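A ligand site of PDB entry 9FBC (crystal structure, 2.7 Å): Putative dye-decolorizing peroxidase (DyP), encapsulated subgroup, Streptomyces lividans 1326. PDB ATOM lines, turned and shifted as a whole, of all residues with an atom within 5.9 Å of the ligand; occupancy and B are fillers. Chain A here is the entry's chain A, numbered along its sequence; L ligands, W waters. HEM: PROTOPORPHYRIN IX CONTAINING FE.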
ATOM      1  N   ASP A 146     -16.002  16.856   6.973  1.00  0.00           N
ATOM      2  CA  ASP A 146     -15.319  15.591   7.077  1.00  0.00           C
ATOM      3  C   ASP A 146     -13.872  15.914   7.351  1.00  0.00           C
ATOM      4  O   ASP A 146     -13.511  17.038   7.719  1.00  0.00           O
ATOM      5  CB  ASP A 146     -15.506  14.755   5.830  1.00  0.00           C
ATOM      6  CG  ASP A 146     -15.122  15.465   4.560  1.00  0.00           C
ATOM      7  OD1 ASP A 146     -14.255  16.346   4.654  1.00  0.00           O
ATOM      8  OD2 ASP A 146     -15.764  15.159   3.541  1.00  0.00           O
ATOM      9  N   MET A 147     -13.050  14.887   7.199  1.00  0.00           N
ATOM     10  CA  MET A 147     -11.675  14.994   7.658  1.00  0.00           C
ATOM     11  C   MET A 147     -10.858  15.792   6.653  1.00  0.00           C
ATOM     12  O   MET A 147      -9.767  16.235   6.966  1.00  0.00           O
ATOM     13  CB  MET A 147     -11.083  13.613   7.947  1.00  0.00           C
ATOM     14  CG  MET A 147     -10.075  13.707   9.058  1.00  0.00           C
ATOM     15  SD  MET A 147     -10.788  14.192  10.651  1.00  0.00           S
ATOM     16  CE  MET A 147     -10.687  12.511  11.308  1.00  0.00           C
ATOM     17  N   LEU A 148     -11.350  16.028   5.454  1.00  0.00           N
ATOM     18  CA  LEU A 148     -10.647  16.883   4.507  1.00  0.00           C
ATOM     19  C   LEU A 148     -11.035  18.343   4.719  1.00  0.00           C
ATOM     20  O   LEU A 148     -10.480  19.228   4.065  1.00  0.00           O
ATOM     21  CB  LEU A 148     -10.959  16.445   3.097  1.00  0.00           C
ATOM     22  CG  LEU A 148     -10.540  15.021   2.771  1.00  0.00           C
ATOM     23  CD1 LEU A 148     -10.958  14.743   1.364  1.00  0.00           C
ATOM     24  CD2 LEU A 148      -9.050  14.778   2.908  1.00  0.00           C
ATOM     25  N   PHE A 150     -14.192  19.640   4.289  1.00  0.00           N
ATOM     26  CA  PHE A 150     -15.301  20.081   3.460  1.00  0.00           C
ATOM     27  C   PHE A 150     -16.660  19.569   3.946  1.00  0.00           C
ATOM     28  O   PHE A 150     -16.760  18.543   4.613  1.00  0.00           O
ATOM     29  CB  PHE A 150     -15.207  19.470   2.054  1.00  0.00           C
ATOM     30  CG  PHE A 150     -14.279  20.237   1.166  1.00  0.00           C
ATOM     31  CD1 PHE A 150     -12.932  20.210   1.415  1.00  0.00           C
ATOM     32  CD2 PHE A 150     -14.755  21.023   0.126  1.00  0.00           C
ATOM     33  CE1 PHE A 150     -12.056  20.913   0.577  1.00  0.00           C
ATOM     34  CE2 PHE A 150     -13.879  21.729  -0.690  1.00  0.00           C
ATOM     35  CZ  PHE A 150     -12.531  21.680  -0.460  1.00  0.00           C
ATOM     36  N   VAL A 151     -17.716  20.267   3.550  1.00  0.00           N
ATOM     37  CA  VAL A 151     -19.024  19.902   4.064  1.00  0.00           C
ATOM     38  C   VAL A 151     -19.481  18.651   3.326  1.00  0.00           C
ATOM     39  O   VAL A 151     -19.377  18.630   2.081  1.00  0.00           O
ATOM     40  CB  VAL A 151     -20.001  21.096   3.866  1.00  0.00           C
ATOM     41  CG1 VAL A 151     -21.374  20.817   4.426  1.00  0.00           C
ATOM     42  CG2 VAL A 151     -19.465  22.382   4.482  1.00  0.00           C
ATOM     43  N   ASP A 152     -19.993  17.662   4.094  1.00  0.00           N
ATOM     44  CA  ASP A 152     -20.170  16.262   3.677  1.00  0.00           C
ATOM     45  C   ASP A 152     -21.587  15.792   3.981  1.00  0.00           C
ATOM     46  O   ASP A 152     -21.957  15.473   5.148  1.00  0.00           O
ATOM     47  CB  ASP A 152     -19.132  15.336   4.311  1.00  0.00           C
ATOM     48  CG  ASP A 152     -19.053  13.918   3.744  1.00  0.00           C
ATOM     49  OD1 ASP A 152     -20.142  13.373   3.422  1.00  0.00           O
ATOM     50  OD2 ASP A 152     -17.918  13.327   3.691  1.00  0.00           O
ATOM     51  N   GLY A 153     -22.319  15.714   2.873  1.00  0.00           N
ATOM     52  CA  GLY A 153     -23.710  15.284   2.891  1.00  0.00           C
ATOM     53  C   GLY A 153     -24.630  16.132   1.989  1.00  0.00           C
ATOM     54  O   GLY A 153     -25.796  15.811   1.892  1.00  0.00           O
ATOM     55  N   THR A 154     -24.133  17.204   1.371  1.00  0.00           N
ATOM     56  CA  THR A 154     -24.975  18.345   1.000  1.00  0.00           C
ATOM     57  C   THR A 154     -25.968  17.971  -0.088  1.00  0.00           C
ATOM     58  O   THR A 154     -27.134  18.302   0.053  1.00  0.00           O
ATOM     59  CB  THR A 154     -24.100  19.519   0.549  1.00  0.00           C
ATOM     60  OG1 THR A 154     -23.178  19.906   1.598  1.00  0.00           O
ATOM     61  CG2 THR A 154     -24.925  20.741   0.174  1.00  0.00           C
ATOM     62  N   GLU A 155     -25.502  17.288  -1.147  1.00  0.00           N
ATOM     63  CA  GLU A 155     -26.353  16.957  -2.304  1.00  0.00           C
ATOM     64  C   GLU A 155     -27.045  15.579  -2.161  1.00  0.00           C
ATOM     65  O   GLU A 155     -27.606  15.041  -3.119  1.00  0.00           O
ATOM     66  CB  GLU A 155     -25.566  16.993  -3.604  1.00  0.00           C
ATOM     67  CG  GLU A 155     -25.263  18.399  -4.118  1.00  0.00           C
ATOM     68  CD  GLU A 155     -26.253  18.723  -5.210  1.00  0.00           C
ATOM     69  OE1 GLU A 155     -26.131  18.465  -6.491  1.00  0.00           O
ATOM     70  OE2 GLU A 155     -27.256  19.189  -4.586  1.00  0.00           O
ATOM     71  N   ASN A 156     -27.061  15.009  -0.960  1.00  0.00           N
ATOM     72  CA  ASN A 156     -27.905  13.855  -0.711  1.00  0.00           C
ATOM     73  C   ASN A 156     -29.361  14.197  -0.934  1.00  0.00           C
ATOM     74  O   ASN A 156     -29.804  15.261  -0.515  1.00  0.00           O
ATOM     75  CB  ASN A 156     -27.851  13.341   0.722  1.00  0.00           C
ATOM     76  CG  ASN A 156     -26.769  12.302   0.930  1.00  0.00           C
ATOM     77  OD1 ASN A 156     -26.426  11.498   0.028  1.00  0.00           O
ATOM     78  ND2 ASN A 156     -26.190  12.359   2.121  1.00  0.00           N
ATOM     79  N   GLN A 184     -17.003   1.302   2.727  1.00  0.00           N
ATOM     80  CA  GLN A 184     -15.563   1.323   2.530  1.00  0.00           C
ATOM     81  C   GLN A 184     -14.941   2.142   3.673  1.00  0.00           C
ATOM     82  O   GLN A 184     -15.375   3.243   3.933  1.00  0.00           O
ATOM     83  CB  GLN A 184     -15.159   1.974   1.210  1.00  0.00           C
ATOM     84  CG  GLN A 184     -15.671   1.247  -0.013  1.00  0.00           C
ATOM     85  CD  GLN A 184     -15.128   1.831  -1.264  1.00  0.00           C
ATOM     86  OE1 GLN A 184     -15.575   2.913  -1.675  1.00  0.00           O
ATOM     87  NE2 GLN A 184     -14.160   1.109  -1.836  1.00  0.00           N
ATOM     88  N   TYR A 186     -11.974   4.456   4.548  1.00  0.00           N
ATOM     89  CA  TYR A 186     -10.978   5.194   3.801  1.00  0.00           C
ATOM     90  C   TYR A 186     -10.103   5.909   4.815  1.00  0.00           C
ATOM     91  O   TYR A 186     -10.601   6.364   5.844  1.00  0.00           O
ATOM     92  CB  TYR A 186     -11.541   6.257   2.859  1.00  0.00           C
ATOM     93  CG  TYR A 186     -12.111   5.774   1.527  1.00  0.00           C
ATOM     94  CD1 TYR A 186     -11.282   5.710   0.432  1.00  0.00           C
ATOM     95  CD2 TYR A 186     -13.465   5.475   1.331  1.00  0.00           C
ATOM     96  CE1 TYR A 186     -11.743   5.352  -0.828  1.00  0.00           C
ATOM     97  CE2 TYR A 186     -13.951   5.039   0.092  1.00  0.00           C
ATOM     98  CZ  TYR A 186     -13.091   5.025  -1.006  1.00  0.00           C
ATOM     99  OH  TYR A 186     -13.497   4.580  -2.248  1.00  0.00           O
ATOM    100  N   HIS A 188      -6.896   8.925   5.072  1.00  0.00           N
ATOM    101  CA  HIS A 188      -6.382  10.080   4.337  1.00  0.00           C
ATOM    102  C   HIS A 188      -4.902  10.289   4.656  1.00  0.00           C
ATOM    103  O   HIS A 188      -4.499  10.001   5.794  1.00  0.00           O
ATOM    104  CB  HIS A 188      -7.319  11.246   4.627  1.00  0.00           C
ATOM    105  CG  HIS A 188      -8.768  11.019   4.316  1.00  0.00           C
ATOM    106  ND1 HIS A 188      -9.255  11.019   3.017  1.00  0.00           N
ATOM    107  CD2 HIS A 188      -9.852  10.845   5.133  1.00  0.00           C
ATOM    108  CE1 HIS A 188     -10.570  10.833   3.039  1.00  0.00           C
ATOM    109  NE2 HIS A 188     -10.978  10.805   4.339  1.00  0.00           N
ATOM    110  N   ILE A 205     -12.374  18.521  -5.146  1.00  0.00           N
ATOM    111  CA  ILE A 205     -13.690  18.139  -4.678  1.00  0.00           C
ATOM    112  C   ILE A 205     -14.759  18.618  -5.662  1.00  0.00           C
ATOM    113  O   ILE A 205     -15.634  17.861  -6.014  1.00  0.00           O
ATOM    114  CB  ILE A 205     -13.941  18.747  -3.273  1.00  0.00           C
ATOM    115  CG1 ILE A 205     -12.956  18.261  -2.252  1.00  0.00           C
ATOM    116  CG2 ILE A 205     -15.399  18.547  -2.846  1.00  0.00           C
ATOM    117  CD1 ILE A 205     -13.228  16.869  -1.780  1.00  0.00           C
ATOM    118  N   ARG A 207     -16.372  21.765  -5.085  1.00  0.00           N
ATOM    119  CA  ARG A 207     -17.158  22.772  -4.392  1.00  0.00           C
ATOM    120  C   ARG A 207     -16.229  23.688  -3.593  1.00  0.00           C
ATOM    121  O   ARG A 207     -15.043  23.393  -3.423  1.00  0.00           O
ATOM    122  CB  ARG A 207     -18.085  22.115  -3.371  1.00  0.00           C
ATOM    123  CG  ARG A 207     -18.905  20.897  -3.768  1.00  0.00           C
ATOM    124  CD  ARG A 207     -19.764  20.419  -2.579  1.00  0.00           C
ATOM    125  NE  ARG A 207     -20.944  21.278  -2.417  1.00  0.00           N
ATOM    126  CZ  ARG A 207     -22.035  21.275  -3.176  1.00  0.00           C
ATOM    127  NH1 ARG A 207     -22.191  20.414  -4.188  1.00  0.00           N
ATOM    128  NH2 ARG A 207     -22.958  22.171  -2.865  1.00  0.00           N
ATOM    129  N   ASP A 212     -19.396  26.126   0.677  1.00  0.00           N
ATOM    130  CA  ASP A 212     -20.032  24.901   0.205  1.00  0.00           C
ATOM    131  C   ASP A 212     -20.975  25.100  -0.981  1.00  0.00           C
ATOM    132  O   ASP A 212     -21.930  24.338  -1.147  1.00  0.00           O
ATOM    133  CB  ASP A 212     -20.797  24.190   1.316  1.00  0.00           C
ATOM    134  CG  ASP A 212     -21.223  22.753   1.093  1.00  0.00           C
ATOM    135  OD1 ASP A 212     -20.405  21.938   0.457  1.00  0.00           O
ATOM    136  OD2 ASP A 212     -22.318  22.474   1.682  1.00  0.00           O
ATOM    137  N   GLU A 214     -21.429  24.897  -5.220  1.00  0.00           N
ATOM    138  CA  GLU A 214     -20.880  24.152  -6.365  1.00  0.00           C
ATOM    139  C   GLU A 214     -19.950  25.063  -7.170  1.00  0.00           C
ATOM    140  O   GLU A 214     -20.207  26.234  -7.281  1.00  0.00           O
ATOM    141  CB  GLU A 214     -22.040  23.571  -7.192  1.00  0.00           C
ATOM    142  CG  GLU A 214     -21.661  22.367  -8.065  1.00  0.00           C
ATOM    143  CD  GLU A 214     -22.718  21.368  -8.523  1.00  0.00           C
ATOM    144  OE1 GLU A 214     -23.285  20.434  -7.857  1.00  0.00           O
ATOM    145  OE2 GLU A 214     -22.869  21.578  -9.748  1.00  0.00           O
ATOM    146  N   HIS A 225     -14.171  15.120  -7.719  1.00  0.00           N
ATOM    147  CA  HIS A 225     -15.046  14.132  -7.101  1.00  0.00           C
ATOM    148  C   HIS A 225     -16.509  14.354  -7.514  1.00  0.00           C
ATOM    149  O   HIS A 225     -17.177  13.370  -7.855  1.00  0.00           O
ATOM    150  CB  HIS A 225     -14.873  14.139  -5.578  1.00  0.00           C
ATOM    151  CG  HIS A 225     -15.680  13.123  -4.820  1.00  0.00           C
ATOM    152  ND1 HIS A 225     -15.580  11.775  -5.058  1.00  0.00           N
ATOM    153  CD2 HIS A 225     -16.605  13.246  -3.792  1.00  0.00           C
ATOM    154  CE1 HIS A 225     -16.400  11.129  -4.188  1.00  0.00           C
ATOM    155  NE2 HIS A 225     -17.040  12.007  -3.425  1.00  0.00           N
ATOM    156  N   VAL A 226     -17.004  15.610  -7.499  1.00  0.00           N
ATOM    157  CA  VAL A 226     -18.415  15.903  -7.715  1.00  0.00           C
ATOM    158  C   VAL A 226     -18.771  15.658  -9.185  1.00  0.00           C
ATOM    159  O   VAL A 226     -19.924  15.389  -9.543  1.00  0.00           O
ATOM    160  CB  VAL A 226     -18.829  17.320  -7.239  1.00  0.00           C
ATOM    161  CG1 VAL A 226     -19.756  18.056  -8.220  1.00  0.00           C
ATOM    162  CG2 VAL A 226     -19.448  17.357  -5.818  1.00  0.00           C
ATOM    163  N   THR A 229     -19.002  11.693  -9.774  1.00  0.00           N
ATOM    164  CA  THR A 229     -20.044  11.003  -9.034  1.00  0.00           C
ATOM    165  C   THR A 229     -21.437  11.560  -9.379  1.00  0.00           C
ATOM    166  O   THR A 229     -22.434  11.055  -8.834  1.00  0.00           O
ATOM    167  CB  THR A 229     -19.710  11.052  -7.525  1.00  0.00           C
ATOM    168  OG1 THR A 229     -19.613  12.408  -7.120  1.00  0.00           O
ATOM    169  CG2 THR A 229     -18.364  10.412  -7.181  1.00  0.00           C
ATOM    170  N   SER A 230     -21.547  12.594 -10.234  1.00  0.00           N
ATOM    171  CA  SER A 230     -22.783  12.909 -10.941  1.00  0.00           C
ATOM    172  C   SER A 230     -22.880  11.976 -12.173  1.00  0.00           C
ATOM    173  O   SER A 230     -22.067  12.060 -13.082  1.00  0.00           O
ATOM    174  CB  SER A 230     -22.899  14.416 -11.332  1.00  0.00           C
ATOM    175  OG  SER A 230     -23.654  15.204 -10.411  1.00  0.00           O
ATOM    176  N   ILE A 241     -27.700   8.179  -4.788  1.00  0.00           N
ATOM    177  CA  ILE A 241     -27.608   7.337  -3.596  1.00  0.00           C
ATOM    178  C   ILE A 241     -27.707   8.188  -2.339  1.00  0.00           C
ATOM    179  O   ILE A 241     -27.647   9.431  -2.356  1.00  0.00           O
ATOM    180  CB  ILE A 241     -26.281   6.562  -3.548  1.00  0.00           C
ATOM    181  CG1 ILE A 241     -25.092   7.467  -3.339  1.00  0.00           C
ATOM    182  CG2 ILE A 241     -26.070   5.716  -4.783  1.00  0.00           C
ATOM    183  CD1 ILE A 241     -23.797   6.710  -3.163  1.00  0.00           C
ATOM    184  N   ARG A 243     -25.757   8.738   1.303  1.00  0.00           N
ATOM    185  CA  ARG A 243     -24.528   8.572   2.065  1.00  0.00           C
ATOM    186  C   ARG A 243     -24.674   9.106   3.500  1.00  0.00           C
ATOM    187  O   ARG A 243     -25.458  10.024   3.731  1.00  0.00           O
ATOM    188  CB  ARG A 243     -23.450   9.426   1.400  1.00  0.00           C
ATOM    189  CG  ARG A 243     -23.038   9.034  -0.010  1.00  0.00           C
ATOM    190  CD  ARG A 243     -22.110  10.063  -0.629  1.00  0.00           C
ATOM    191  NE  ARG A 243     -22.876  11.200  -1.108  1.00  0.00           N
ATOM    192  CZ  ARG A 243     -22.661  12.455  -0.719  1.00  0.00           C
ATOM    193  NH1 ARG A 243     -21.666  12.766   0.084  1.00  0.00           N
ATOM    194  NH2 ARG A 243     -23.436  13.414  -1.167  1.00  0.00           N
ATOM    195  N   ASN A 245     -21.394   9.399   5.435  1.00  0.00           N
ATOM    196  CA  ASN A 245     -19.977   9.432   5.734  1.00  0.00           C
ATOM    197  C   ASN A 245     -19.789  10.025   7.116  1.00  0.00           C
ATOM    198  O   ASN A 245     -20.335  11.111   7.423  1.00  0.00           O
ATOM    199  CB  ASN A 245     -19.153  10.264   4.750  1.00  0.00           C
ATOM    200  CG  ASN A 245     -19.366   9.825   3.323  1.00  0.00           C
ATOM    201  OD1 ASN A 245     -19.871   8.711   3.106  1.00  0.00           O
ATOM    202  ND2 ASN A 245     -18.962  10.640   2.353  1.00  0.00           N
ATOM    203  N   THR A 258     -12.342   8.752   6.777  1.00  0.00           N
ATOM    204  CA  THR A 258     -13.755   8.948   6.516  1.00  0.00           C
ATOM    205  C   THR A 258     -14.302   7.537   6.217  1.00  0.00           C
ATOM    206  O   THR A 258     -13.773   6.826   5.375  1.00  0.00           O
ATOM    207  CB  THR A 258     -13.887  10.004   5.410  1.00  0.00           C
ATOM    208  OG1 THR A 258     -13.879  11.309   6.026  1.00  0.00           O
ATOM    209  CG2 THR A 258     -15.147   9.749   4.611  1.00  0.00           C
ATOM    210  N   PHE A 260     -17.084   5.396   4.711  1.00  0.00           N
ATOM    211  CA  PHE A 260     -18.024   5.673   3.640  1.00  0.00           C
ATOM    212  C   PHE A 260     -19.157   4.661   3.722  1.00  0.00           C
ATOM    213  O   PHE A 260     -18.900   3.473   3.859  1.00  0.00           O
ATOM    214  CB  PHE A 260     -17.354   5.574   2.265  1.00  0.00           C
ATOM    215  CG  PHE A 260     -18.390   5.520   1.157  1.00  0.00           C
ATOM    216  CD1 PHE A 260     -18.995   6.672   0.690  1.00  0.00           C
ATOM    217  CD2 PHE A 260     -18.803   4.309   0.616  1.00  0.00           C
ATOM    218  CE1 PHE A 260     -20.000   6.609  -0.277  1.00  0.00           C
ATOM    219  CE2 PHE A 260     -19.786   4.263  -0.376  1.00  0.00           C
ATOM    220  CZ  PHE A 260     -20.364   5.398  -0.827  1.00  0.00           C
ATOM    221  N   THR A 270     -24.410   2.513  -7.250  1.00  0.00           N
ATOM    222  CA  THR A 270     -23.261   2.726  -6.378  1.00  0.00           C
ATOM    223  C   THR A 270     -22.007   2.244  -7.142  1.00  0.00           C
ATOM    224  O   THR A 270     -20.975   2.923  -7.207  1.00  0.00           O
ATOM    225  CB  THR A 270     -23.476   2.010  -5.043  1.00  0.00           C
ATOM    226  OG1 THR A 270     -24.634   2.190  -4.210  1.00  0.00           O
ATOM    227  CG2 THR A 270     -22.388   2.387  -4.077  1.00  0.00           C
ATOM    228  N   MET A 273     -20.544   4.500  -9.863  1.00  0.00           N
ATOM    229  CA  MET A 273     -19.826   5.641  -9.360  1.00  0.00           C
ATOM    230  C   MET A 273     -18.408   5.221  -8.976  1.00  0.00           C
ATOM    231  O   MET A 273     -17.443   5.922  -9.225  1.00  0.00           O
ATOM    232  CB  MET A 273     -20.585   6.217  -8.164  1.00  0.00           C
ATOM    233  CG  MET A 273     -21.926   6.816  -8.511  1.00  0.00           C
ATOM    234  SD  MET A 273     -22.764   7.032  -6.932  1.00  0.00           S
ATOM    235  CE  MET A 273     -24.093   8.172  -7.382  1.00  0.00           C
ATOM    236  N   LEU A 274     -18.281   4.016  -8.462  1.00  0.00           N
ATOM    237  CA  LEU A 274     -17.009   3.495  -8.059  1.00  0.00           C
ATOM    238  C   LEU A 274     -16.100   3.265  -9.261  1.00  0.00           C
ATOM    239  O   LEU A 274     -14.902   3.525  -9.173  1.00  0.00           O
ATOM    240  CB  LEU A 274     -17.292   2.208  -7.291  1.00  0.00           C
ATOM    241  CG  LEU A 274     -17.735   2.406  -5.826  1.00  0.00           C
ATOM    242  CD1 LEU A 274     -18.315   1.229  -5.088  1.00  0.00           C
ATOM    243  CD2 LEU A 274     -16.587   2.865  -4.931  1.00  0.00           C
ATOM    244  N   MET A 277     -14.777   6.409 -10.332  1.00  0.00           N
ATOM    245  CA  MET A 277     -13.795   6.894  -9.378  1.00  0.00           C
ATOM    246  C   MET A 277     -12.448   6.199  -9.546  1.00  0.00           C
ATOM    247  O   MET A 277     -11.438   6.901  -9.524  1.00  0.00           O
ATOM    248  CB  MET A 277     -14.293   6.724  -7.935  1.00  0.00           C
ATOM    249  CG  MET A 277     -15.326   7.762  -7.541  1.00  0.00           C
ATOM    250  SD  MET A 277     -15.863   7.507  -5.846  1.00  0.00           S
ATOM    251  CE  MET A 277     -14.312   7.938  -5.059  1.00  0.00           C
ATOM    252  N   ILE A 289      -9.719  12.557  -5.572  1.00  0.00           N
ATOM    253  CA  ILE A 289      -9.832  12.383  -4.137  1.00  0.00           C
ATOM    254  C   ILE A 289      -9.029  11.164  -3.673  1.00  0.00           C
ATOM    255  O   ILE A 289      -8.679  11.071  -2.509  1.00  0.00           O
ATOM    256  CB  ILE A 289     -11.316  12.305  -3.706  1.00  0.00           C
ATOM    257  CG1 ILE A 289     -11.480  12.614  -2.215  1.00  0.00           C
ATOM    258  CG2 ILE A 289     -11.923  10.957  -4.055  1.00  0.00           C
ATOM    259  CD1 ILE A 289     -12.887  12.955  -1.769  1.00  0.00           C
ATOM    260  N   LEU A 290      -8.741  10.228  -4.573  1.00  0.00           N
ATOM    261  CA  LEU A 290      -8.116   8.972  -4.194  1.00  0.00           C
ATOM    262  C   LEU A 290      -6.621   9.161  -4.081  1.00  0.00           C
ATOM    263  O   LEU A 290      -5.907   8.343  -3.492  1.00  0.00           O
ATOM    264  CB  LEU A 290      -8.434   7.945  -5.278  1.00  0.00           C
ATOM    265  CG  LEU A 290      -9.907   7.577  -5.378  1.00  0.00           C
ATOM    266  CD1 LEU A 290     -10.257   6.612  -6.520  1.00  0.00           C
ATOM    267  CD2 LEU A 290     -10.358   7.072  -4.012  1.00  0.00           C
ATOM    268  N   SER A 293      -6.684   9.466  -0.446  1.00  0.00           N
ATOM    269  CA  SER A 293      -7.606   8.625   0.285  1.00  0.00           C
ATOM    270  C   SER A 293      -7.349   7.198  -0.167  1.00  0.00           C
ATOM    271  O   SER A 293      -7.303   6.961  -1.366  1.00  0.00           O
ATOM    272  CB  SER A 293      -9.041   9.000   0.012  1.00  0.00           C
ATOM    273  OG  SER A 293      -9.240  10.408   0.055  1.00  0.00           O
HETATM  274  CHA HEM L   1     -20.179  14.314  -2.911  1.00  0.00           C
HETATM  275  CHB HEM L   1     -16.705  13.619   0.379  1.00  0.00           C
HETATM  276  CHC HEM L   1     -16.234   9.045  -1.080  1.00  0.00           C
HETATM  277  CHD HEM L   1     -20.304   9.757  -3.624  1.00  0.00           C
HETATM  278  C1A HEM L   1     -19.203  14.457  -1.947  1.00  0.00           C
HETATM  279  C2A HEM L   1     -18.974  15.718  -1.383  1.00  0.00           C
HETATM  280  C3A HEM L   1     -18.014  15.511  -0.458  1.00  0.00           C
HETATM  281  C4A HEM L   1     -17.650  14.167  -0.438  1.00  0.00           C
HETATM  282  CMA HEM L   1     -17.455  16.600   0.400  1.00  0.00           C
HETATM  283  CAA HEM L   1     -19.633  17.065  -1.757  1.00  0.00           C
HETATM  284  CBA HEM L   1     -20.621  17.445  -0.695  1.00  0.00           C
HETATM  285  CGA HEM L   1     -21.752  16.564  -1.093  1.00  0.00           C
HETATM  286  O1A HEM L   1     -22.143  15.745  -0.219  1.00  0.00           O
HETATM  287  O2A HEM L   1     -22.143  16.695  -2.340  1.00  0.00           O
HETATM  288  C1B HEM L   1     -16.258  12.324   0.242  1.00  0.00           C
HETATM  289  C2B HEM L   1     -15.130  11.856   0.949  1.00  0.00           C
HETATM  290  C3B HEM L   1     -14.978  10.589   0.568  1.00  0.00           C
HETATM  291  C4B HEM L   1     -16.054  10.263  -0.387  1.00  0.00           C
HETATM  292  CMB HEM L   1     -14.254  12.504   1.996  1.00  0.00           C
HETATM  293  CAB HEM L   1     -13.845   9.840   1.090  1.00  0.00           C
HETATM  294  CBB HEM L   1     -13.402   8.753   0.516  1.00  0.00           C
HETATM  295  C1C HEM L   1     -17.283   8.765  -1.938  1.00  0.00           C
HETATM  296  C2C HEM L   1     -17.624   7.544  -2.554  1.00  0.00           C
HETATM  297  C3C HEM L   1     -18.805   7.768  -3.265  1.00  0.00           C
HETATM  298  C4C HEM L   1     -19.160   9.153  -3.083  1.00  0.00           C
HETATM  299  CMC HEM L   1     -16.913   6.245  -2.408  1.00  0.00           C
HETATM  300  CAC HEM L   1     -19.654   6.880  -4.095  1.00  0.00           C
HETATM  301  CBC HEM L   1     -19.462   5.608  -4.308  1.00  0.00           C
HETATM  302  C1D HEM L   1     -20.622  11.073  -3.639  1.00  0.00           C
HETATM  303  C2D HEM L   1     -21.782  11.603  -4.405  1.00  0.00           C
HETATM  304  C3D HEM L   1     -21.765  12.959  -4.267  1.00  0.00           C
HETATM  305  C4D HEM L   1     -20.574  13.089  -3.350  1.00  0.00           C
HETATM  306  CMD HEM L   1     -22.771  10.795  -5.216  1.00  0.00           C
HETATM  307  CAD HEM L   1     -22.753  14.038  -4.828  1.00  0.00           C
HETATM  308  CBD HEM L   1     -23.049  14.350  -6.367  1.00  0.00           C
HETATM  309  CGD HEM L   1     -23.814  15.680  -6.839  1.00  0.00           C
HETATM  310  O1D HEM L   1     -24.919  15.697  -7.596  1.00  0.00           O
HETATM  311  O2D HEM L   1     -23.233  16.773  -6.433  1.00  0.00           O
HETATM  312  NA  HEM L   1     -18.365  13.510  -1.356  1.00  0.00           N
HETATM  313  NB  HEM L   1     -16.805  11.363  -0.503  1.00  0.00           N
HETATM  314  NC  HEM L   1     -18.236   9.657  -2.263  1.00  0.00           N
HETATM  315  ND  HEM L   1     -19.893  11.939  -3.014  1.00  0.00           N
HETATM  316 FE   HEM L   1     -18.397  11.579  -1.830  1.00  0.00          FE
HETATM  317  O   HOH W   1     -26.214  17.795  -8.883  1.00  0.00           O
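The side-chain carboxylate of Glu 155 lies close to an oxygen (O1D) of the ligand (3.2 Å).
Residues that only touch the ligand: Val 151 (3.3 Å), Tyr 186 (3.4 Å), Phe 260 (3.4 Å), Asp 146 (3.4 Å), Arg 207 (3.5 Å), Asp 152 (3.5 Å), Thr 229 (3.6 Å), Met 273 (3.6 Å), Asn 245 (3.7 Å), Gln 184 (3.7 Å), Ile 289 (3.7 Å), Met 277 (3.7 Å), Thr 258 (3.8 Å), Val 226 (3.9 Å), Glu 214 (3.9 Å), His 188 (3.9 Å) and Leu 274 (3.9 Å).
Hydrophobic or aromatic side chains within 4 Å of the ligand: Tyr 186, His 188, His 225, Val 226, Phe 260, Met 273, Leu 274, Met 277 and Ile 289.
Of the 33 residues printed, 23 come within 4 Å of the ligand.
The nearest printed residue that does not touch the ligand is Phe 150 (4.003 Å).
O of Gly 153 sits close to ND2 of Asn 156 (3.5 Å).
The backbone NH of Tyr 186 sits at hydrogen-bond distance from the backbone carbonyl oxygen of Thr 258, at 3.1 Å.
OD1 of Asp 146 is in hydrogen-bond range of N of Phe 150 (3.3 Å).
OD1 of Asp 146 lies within hydrogen-bond range of N of Leu 148.
The guanidinium group (NE) of Arg 207 lies within salt-bridge range of the side-chain carboxylate (OD1) of Asp 212 (3.0 Å).
O of Ile 289 lies within hydrogen-bond range of OG of Ser 293 (2.7 Å).
N of Val 226 is in hydrogen-bond range of O of Ile 205 (3.0 Å).
OG of Ser 293 lies within hydrogen-bond range of ND1 of His 188 (3.0 Å).
Water W1 lies within hydrogen-bond range of the side-chain carboxylate of Glu 155 (2.5 Å) and an oxygen (O1D) of the ligand (2.8 Å).
NE2 of His 225 binds FE of the ligand (2.1 Å).
The guanidinium group of Arg 243 lies within salt-bridge range of an oxygen (O1A) of the ligand (2.8 Å).
The backbone NH of Thr 154 lies within hydrogen-bond range of an oxygen (O1A) of the ligand, 2.9 Å away.
An oxygen (O1A) of the ligand lies within hydrogen-bond range of the backbone NH (N) of Gly 153 (3.1 Å).
O1D of the ligand is in hydrogen-bond range of OG of Ser 230 (3.1 Å).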
